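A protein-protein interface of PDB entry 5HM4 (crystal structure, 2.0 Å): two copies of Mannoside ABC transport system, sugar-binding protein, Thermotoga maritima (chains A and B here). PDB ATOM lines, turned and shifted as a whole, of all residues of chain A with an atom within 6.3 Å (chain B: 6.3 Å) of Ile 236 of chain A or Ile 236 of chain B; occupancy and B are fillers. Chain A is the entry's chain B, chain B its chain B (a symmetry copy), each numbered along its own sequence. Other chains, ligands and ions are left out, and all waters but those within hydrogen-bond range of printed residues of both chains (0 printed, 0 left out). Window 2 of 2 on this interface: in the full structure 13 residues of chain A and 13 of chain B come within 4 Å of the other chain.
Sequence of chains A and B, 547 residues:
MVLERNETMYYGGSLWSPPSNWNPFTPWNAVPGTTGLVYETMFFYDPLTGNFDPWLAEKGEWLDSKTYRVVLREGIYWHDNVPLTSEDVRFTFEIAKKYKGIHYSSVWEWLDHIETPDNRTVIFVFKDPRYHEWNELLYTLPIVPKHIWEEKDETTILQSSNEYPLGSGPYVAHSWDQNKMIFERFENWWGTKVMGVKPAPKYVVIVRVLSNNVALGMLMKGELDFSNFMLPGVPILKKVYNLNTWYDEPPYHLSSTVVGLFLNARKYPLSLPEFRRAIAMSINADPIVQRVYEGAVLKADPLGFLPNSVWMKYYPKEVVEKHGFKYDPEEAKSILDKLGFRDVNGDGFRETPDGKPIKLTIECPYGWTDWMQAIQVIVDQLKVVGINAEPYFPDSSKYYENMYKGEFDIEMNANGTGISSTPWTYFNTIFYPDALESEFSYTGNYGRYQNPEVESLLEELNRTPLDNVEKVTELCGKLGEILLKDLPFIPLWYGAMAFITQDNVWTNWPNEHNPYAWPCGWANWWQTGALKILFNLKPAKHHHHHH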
ATOM      1  N   PRO A 232      32.236 -10.262  30.477  1.00  0.00           N
ATOM      2  CA  PRO A 232      31.036 -11.083  30.656  1.00  0.00           C
ATOM      3  C   PRO A 232      30.707 -11.870  29.395  1.00  0.00           C
ATOM      4  O   PRO A 232      31.151 -11.548  28.291  1.00  0.00           O
ATOM      5  CB  PRO A 232      29.949 -10.051  30.972  1.00  0.00           C
ATOM      6  CG  PRO A 232      30.446  -8.800  30.324  1.00  0.00           C
ATOM      7  CD  PRO A 232      31.930  -8.825  30.400  1.00  0.00           C
ATOM      8  N   GLY A 233      29.919 -12.925  29.579  1.00  0.00           N
ATOM      9  CA  GLY A 233      29.494 -13.746  28.463  1.00  0.00           C
ATOM     10  C   GLY A 233      30.398 -14.913  28.144  1.00  0.00           C
ATOM     11  O   GLY A 233      30.458 -15.337  26.984  1.00  0.00           O
ATOM     12  N   VAL A 234      31.087 -15.465  29.148  1.00  0.00           N
ATOM     13  CA  VAL A 234      32.109 -16.482  28.878  1.00  0.00           C
ATOM     14  C   VAL A 234      31.540 -17.758  28.270  1.00  0.00           C
ATOM     15  O   VAL A 234      32.151 -18.285  27.328  1.00  0.00           O
ATOM     16  CB  VAL A 234      32.936 -16.745  30.143  1.00  0.00           C
ATOM     17  N   PRO A 235      30.424 -18.329  28.751  1.00  0.00           N
ATOM     18  CA  PRO A 235      29.952 -19.598  28.160  1.00  0.00           C
ATOM     19  C   PRO A 235      29.780 -19.546  26.652  1.00  0.00           C
ATOM     20  O   PRO A 235      30.281 -20.420  25.933  1.00  0.00           O
ATOM     21  CB  PRO A 235      28.611 -19.828  28.872  1.00  0.00           C
ATOM     22  CG  PRO A 235      28.761 -19.149  30.169  1.00  0.00           C
ATOM     23  CD  PRO A 235      29.586 -17.930  29.899  1.00  0.00           C
ATOM     24  N   ILE A 236      29.095 -18.517  26.154  1.00  0.00           N
ATOM     25  CA  ILE A 236      28.783 -18.425  24.733  1.00  0.00           C
ATOM     26  C   ILE A 236      30.038 -18.108  23.929  1.00  0.00           C
ATOM     27  O   ILE A 236      30.162 -18.524  22.770  1.00  0.00           O
ATOM     28  CB  ILE A 236      27.669 -17.383  24.503  1.00  0.00           C
ATOM     29  CG1 ILE A 236      26.480 -17.623  25.446  1.00  0.00           C
ATOM     30  CG2 ILE A 236      27.192 -17.408  23.061  1.00  0.00           C
ATOM     31  CD1 ILE A 236      26.588 -16.958  26.818  1.00  0.00           C
ATOM     32  N   LEU A 237      30.985 -17.378  24.521  1.00  0.00           N
ATOM     33  CA  LEU A 237      32.267 -17.150  23.861  1.00  0.00           C
ATOM     34  C   LEU A 237      32.994 -18.467  23.620  1.00  0.00           C
ATOM     35  O   LEU A 237      33.393 -18.771  22.490  1.00  0.00           O
ATOM     36  CB  LEU A 237      33.126 -16.202  24.698  1.00  0.00           C
ATOM     37  N   LYS A 238      33.171 -19.266  24.677  1.00  0.00           N
ATOM     38  CA  LYS A 238      33.783 -20.582  24.525  1.00  0.00           C
ATOM     39  C   LYS A 238      32.984 -21.451  23.565  1.00  0.00           C
ATOM     40  O   LYS A 238      33.546 -22.075  22.659  1.00  0.00           O
ATOM     41  CB  LYS A 238      33.892 -21.275  25.884  1.00  0.00           C
ATOM     42  CG  LYS A 238      34.832 -20.614  26.873  1.00  0.00           C
ATOM     43  CD  LYS A 238      35.004 -21.484  28.109  1.00  0.00           C
ATOM     44  CE  LYS A 238      35.589 -22.848  27.763  1.00  0.00           C
ATOM     45  NZ  LYS A 238      37.069 -22.884  27.936  1.00  0.00           N
ATOM     46  N   LYS A 239      31.663 -21.498  23.754  1.00  0.00           N
ATOM     47  CA  LYS A 239      30.830 -22.402  22.969  1.00  0.00           C
ATOM     48  C   LYS A 239      30.951 -22.127  21.477  1.00  0.00           C
ATOM     49  O   LYS A 239      31.018 -23.062  20.671  1.00  0.00           O
ATOM     50  CB  LYS A 239      29.371 -22.286  23.415  1.00  0.00           C
ATOM     51  N   VAL A 240      30.994 -20.857  21.084  1.00  0.00           N
ATOM     52  CA  VAL A 240      30.821 -20.508  19.683  1.00  0.00           C
ATOM     53  C   VAL A 240      32.011 -19.775  19.076  1.00  0.00           C
ATOM     54  O   VAL A 240      32.118 -19.726  17.840  1.00  0.00           O
ATOM     55  CB  VAL A 240      29.535 -19.682  19.475  1.00  0.00           C
ATOM     56  CG1 VAL A 240      29.015 -19.912  18.087  1.00  0.00           C
ATOM     57  CG2 VAL A 240      28.475 -20.053  20.501  1.00  0.00           C
ATOM     58  N   TYR A 241      32.925 -19.202  19.863  1.00  0.00           N
ATOM     59  CA  TYR A 241      33.913 -18.301  19.279  1.00  0.00           C
ATOM     60  C   TYR A 241      35.354 -18.686  19.596  1.00  0.00           C
ATOM     61  O   TYR A 241      36.255 -17.859  19.425  1.00  0.00           O
ATOM     62  CB  TYR A 241      33.630 -16.862  19.710  1.00  0.00           C
ATOM     63  CG  TYR A 241      32.414 -16.292  19.022  1.00  0.00           C
ATOM     64  CD1 TYR A 241      32.518 -15.695  17.774  1.00  0.00           C
ATOM     65  CD2 TYR A 241      31.157 -16.373  19.607  1.00  0.00           C
ATOM     66  CE1 TYR A 241      31.410 -15.182  17.131  1.00  0.00           C
ATOM     67  CE2 TYR A 241      30.039 -15.861  18.972  1.00  0.00           C
ATOM     68  CZ  TYR A 241      30.173 -15.268  17.734  1.00  0.00           C
ATOM     69  OH  TYR A 241      29.066 -14.756  17.098  1.00  0.00           O
ATOM     70  N   ASN A 242      35.592 -19.922  20.037  1.00  0.00           N
ATOM     71  CA  ASN A 242      36.941 -20.485  20.137  1.00  0.00           C
ATOM     72  C   ASN A 242      37.837 -19.670  21.068  1.00  0.00           C
ATOM     73  O   ASN A 242      39.026 -19.479  20.804  1.00  0.00           O
ATOM     74  CB  ASN A 242      37.580 -20.622  18.754  1.00  0.00           C
ATOM     75  N   GLU A 294      26.676 -16.049  35.666  1.00  0.00           N
ATOM     76  CA  GLU A 294      26.539 -17.147  34.705  1.00  0.00           C
ATOM     77  C   GLU A 294      27.461 -18.313  35.054  1.00  0.00           C
ATOM     78  O   GLU A 294      28.053 -18.950  34.181  1.00  0.00           O
ATOM     79  CB  GLU A 294      26.793 -16.661  33.278  1.00  0.00           C
ATOM     80  CG  GLU A 294      25.933 -15.484  32.859  1.00  0.00           C
ATOM     81  CD  GLU A 294      26.302 -14.951  31.488  1.00  0.00           C
ATOM     82  OE1 GLU A 294      26.941 -13.879  31.420  1.00  0.00           O
ATOM     83  OE2 GLU A 294      25.960 -15.604  30.480  1.00  0.00           O
ATOM     84  N   PRO B 232      26.253 -15.959  15.440  1.00  0.00           N
ATOM     85  CA  PRO B 232      25.522 -16.549  16.564  1.00  0.00           C
ATOM     86  C   PRO B 232      25.798 -15.802  17.860  1.00  0.00           C
ATOM     87  O   PRO B 232      26.785 -15.077  17.999  1.00  0.00           O
ATOM     88  CB  PRO B 232      26.061 -17.982  16.618  1.00  0.00           C
ATOM     89  CG  PRO B 232      27.422 -17.875  16.012  1.00  0.00           C
ATOM     90  CD  PRO B 232      27.359 -16.810  14.976  1.00  0.00           C
ATOM     91  N   GLY B 233      24.894 -15.984  18.819  1.00  0.00           N
ATOM     92  CA  GLY B 233      25.045 -15.363  20.119  1.00  0.00           C
ATOM     93  C   GLY B 233      24.408 -14.000  20.257  1.00  0.00           C
ATOM     94  O   GLY B 233      24.884 -13.185  21.056  1.00  0.00           O
ATOM     95  N   VAL B 234      23.325 -13.736  19.520  1.00  0.00           N
ATOM     96  CA  VAL B 234      22.766 -12.381  19.478  1.00  0.00           C
ATOM     97  C   VAL B 234      22.238 -11.907  20.825  1.00  0.00           C
ATOM     98  O   VAL B 234      22.493 -10.747  21.184  1.00  0.00           O
ATOM     99  CB  VAL B 234      21.719 -12.279  18.361  1.00  0.00           C
ATOM    100  N   PRO B 235      21.486 -12.702  21.605  1.00  0.00           N
ATOM    101  CA  PRO B 235      20.953 -12.168  22.875  1.00  0.00           C
ATOM    102  C   PRO B 235      22.013 -11.570  23.783  1.00  0.00           C
ATOM    103  O   PRO B 235      21.861 -10.441  24.268  1.00  0.00           O
ATOM    104  CB  PRO B 235      20.295 -13.400  23.512  1.00  0.00           C
ATOM    105  CG  PRO B 235      19.914 -14.247  22.371  1.00  0.00           C
ATOM    106  CD  PRO B 235      20.998 -14.071  21.354  1.00  0.00           C
ATOM    107  N   ILE B 236      23.103 -12.303  24.009  1.00  0.00           N
ATOM    108  CA  ILE B 236      24.134 -11.870  24.944  1.00  0.00           C
ATOM    109  C   ILE B 236      24.918 -10.696  24.372  1.00  0.00           C
ATOM    110  O   ILE B 236      25.399  -9.837  25.123  1.00  0.00           O
ATOM    111  CB  ILE B 236      25.050 -13.057  25.308  1.00  0.00           C
ATOM    112  CG1 ILE B 236      24.228 -14.287  25.722  1.00  0.00           C
ATOM    113  CG2 ILE B 236      26.007 -12.681  26.426  1.00  0.00           C
ATOM    114  CD1 ILE B 236      23.786 -15.196  24.575  1.00  0.00           C
ATOM    115  N   LEU B 237      25.057 -10.631  23.046  1.00  0.00           N
ATOM    116  CA  LEU B 237      25.679  -9.468  22.422  1.00  0.00           C
ATOM    117  C   LEU B 237      24.878  -8.205  22.713  1.00  0.00           C
ATOM    118  O   LEU B 237      25.423  -7.210  23.206  1.00  0.00           O
ATOM    119  CB  LEU B 237      25.812  -9.690  20.916  1.00  0.00           C
ATOM    120  N   LYS B 238      23.576  -8.229  22.416  1.00  0.00           N
ATOM    121  CA  LYS B 238      22.714  -7.095  22.736  1.00  0.00           C
ATOM    122  C   LYS B 238      22.723  -6.804  24.229  1.00  0.00           C
ATOM    123  O   LYS B 238      22.881  -5.653  24.649  1.00  0.00           O
ATOM    124  CB  LYS B 238      21.284  -7.368  22.268  1.00  0.00           C
ATOM    125  CG  LYS B 238      21.103  -7.474  20.768  1.00  0.00           C
ATOM    126  CD  LYS B 238      19.627  -7.557  20.412  1.00  0.00           C
ATOM    127  CE  LYS B 238      18.862  -6.326  20.878  1.00  0.00           C
ATOM    128  NZ  LYS B 238      18.725  -5.306  19.799  1.00  0.00           N
ATOM    129  N   LYS B 239      22.554  -7.846  25.046  1.00  0.00           N
ATOM    130  CA  LYS B 239      22.417  -7.652  26.485  1.00  0.00           C
ATOM    131  C   LYS B 239      23.633  -6.949  27.075  1.00  0.00           C
ATOM    132  O   LYS B 239      23.492  -6.068  27.931  1.00  0.00           O
ATOM    133  CB  LYS B 239      22.193  -8.998  27.175  1.00  0.00           C
ATOM    134  N   VAL B 240      24.832  -7.311  26.629  1.00  0.00           N
ATOM    135  CA  VAL B 240      26.038  -6.904  27.334  1.00  0.00           C
ATOM    136  C   VAL B 240      26.994  -6.068  26.492  1.00  0.00           C
ATOM    137  O   VAL B 240      27.869  -5.399  27.066  1.00  0.00           O
ATOM    138  CB  VAL B 240      26.780  -8.128  27.909  1.00  0.00           C
ATOM    139  CG1 VAL B 240      27.550  -7.716  29.129  1.00  0.00           C
ATOM    140  CG2 VAL B 240      25.806  -9.245  28.256  1.00  0.00           C
ATOM    141  N   TYR B 241      26.886  -6.051  25.162  1.00  0.00           N
ATOM    142  CA  TYR B 241      27.949  -5.453  24.361  1.00  0.00           C
ATOM    143  C   TYR B 241      27.458  -4.373  23.403  1.00  0.00           C
ATOM    144  O   TYR B 241      28.186  -4.009  22.474  1.00  0.00           O
ATOM    145  CB  TYR B 241      28.713  -6.541  23.606  1.00  0.00           C
ATOM    146  CG  TYR B 241      29.592  -7.357  24.521  1.00  0.00           C
ATOM    147  CD1 TYR B 241      30.878  -6.938  24.831  1.00  0.00           C
ATOM    148  CD2 TYR B 241      29.130  -8.534  25.097  1.00  0.00           C
ATOM    149  CE1 TYR B 241      31.685  -7.671  25.677  1.00  0.00           C
ATOM    150  CE2 TYR B 241      29.931  -9.276  25.945  1.00  0.00           C
ATOM    151  CZ  TYR B 241      31.207  -8.839  26.232  1.00  0.00           C
ATOM    152  OH  TYR B 241      32.009  -9.574  27.074  1.00  0.00           O
ATOM    153  N   ASN B 242      26.253  -3.846  23.615  1.00  0.00           N
ATOM    154  CA  ASN B 242      25.777  -2.643  22.925  1.00  0.00           C
ATOM    155  C   ASN B 242      25.749  -2.823  21.408  1.00  0.00           C
ATOM    156  O   ASN B 242      26.075  -1.908  20.651  1.00  0.00           O
ATOM    157  CB  ASN B 242      26.618  -1.425  23.310  1.00  0.00           C
ATOM    158  N   GLU B 294      18.453 -19.940  19.267  1.00  0.00           N
ATOM    159  CA  GLU B 294      18.297 -19.056  20.425  1.00  0.00           C
ATOM    160  C   GLU B 294      17.209 -18.012  20.189  1.00  0.00           C
ATOM    161  O   GLU B 294      17.336 -16.850  20.577  1.00  0.00           O
ATOM    162  CB  GLU B 294      19.624 -18.386  20.786  1.00  0.00           C
ATOM    163  CG  GLU B 294      20.769 -19.355  21.013  1.00  0.00           C
ATOM    164  CD  GLU B 294      22.092 -18.651  21.241  1.00  0.00           C
ATOM    165  OE1 GLU B 294      22.929 -18.643  20.313  1.00  0.00           O
ATOM    166  OE2 GLU B 294      22.294 -18.100  22.344  1.00  0.00           O
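The side-chain hydroxyl (OH) of Tyr 241 of chain B lies within hydrogen-bond range of the backbone carbonyl oxygen (O) of Pro 232 of chain A. The side-chain hydroxyl (OH) of Tyr 241 of chain A is in hydrogen-bond range of the backbone carbonyl oxygen (O) of Pro 232 of chain B, 2.5 Å away.
Pro 232 of chain A touches Val 240 of chain B. Ile 236 of chain A touches Ile 236 of chain B (CD1 to CG1, 3.7 Å). Pro 232 of chain B touches Val 240 of chain A.
Of the printed residues of chain B, Pro 232 of chain A touches Val 240 and Tyr 241. Of the printed residues of chain B, Ile 236 of chain A touches Ile 236 (3.7 Å). Of the printed residues of chain B, Tyr 241 of chain A touches Pro 232 (2.5 Å). Of the printed residues of chain A, Ile 236 of chain B touches Ile 236 (3.7 Å). Of the printed residues of chain A, Val 240 of chain B touches Pro 232 (3.3 Å). Glu 294 of chain B touches none of the printed residues of chain A. The nearest residue of chain B that does not touch Ile 236 of chain A is Gly 233 of chain B (4.2 Å).
Of the 12 printed residues of chain A, 4 touch a printed residue of chain B. Hydrophobic or aromatic side chains of chain A within 4 Å of the printed part of chain B: Pro 232, Ile 236, Val 240 and Tyr 241. Of the 12 printed residues of chain B, 4 touch a printed residue of chain A. Hydrophobic or aromatic side chains of chain B that line the printed part of chain A: Pro 232, Ile 236, Val 240 and Tyr 241.
Pro 232 of chain A touches Val 240 of chain B, and with the chains exchanged Val 240 of chain A touches Pro 232 of chain B. Pro 232 of chain A touches Tyr 241 of chain B, and with the chains exchanged Tyr 241 of chain A touches Pro 232 of chain B. Ile 236 of chain A touches its own counterpart, Ile 236 of chain B. 12 positions are printed for both chains. Of the 5 pairs that touch across the chains among the printed residues, 5 have their exchanged pair printed and touching as well.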
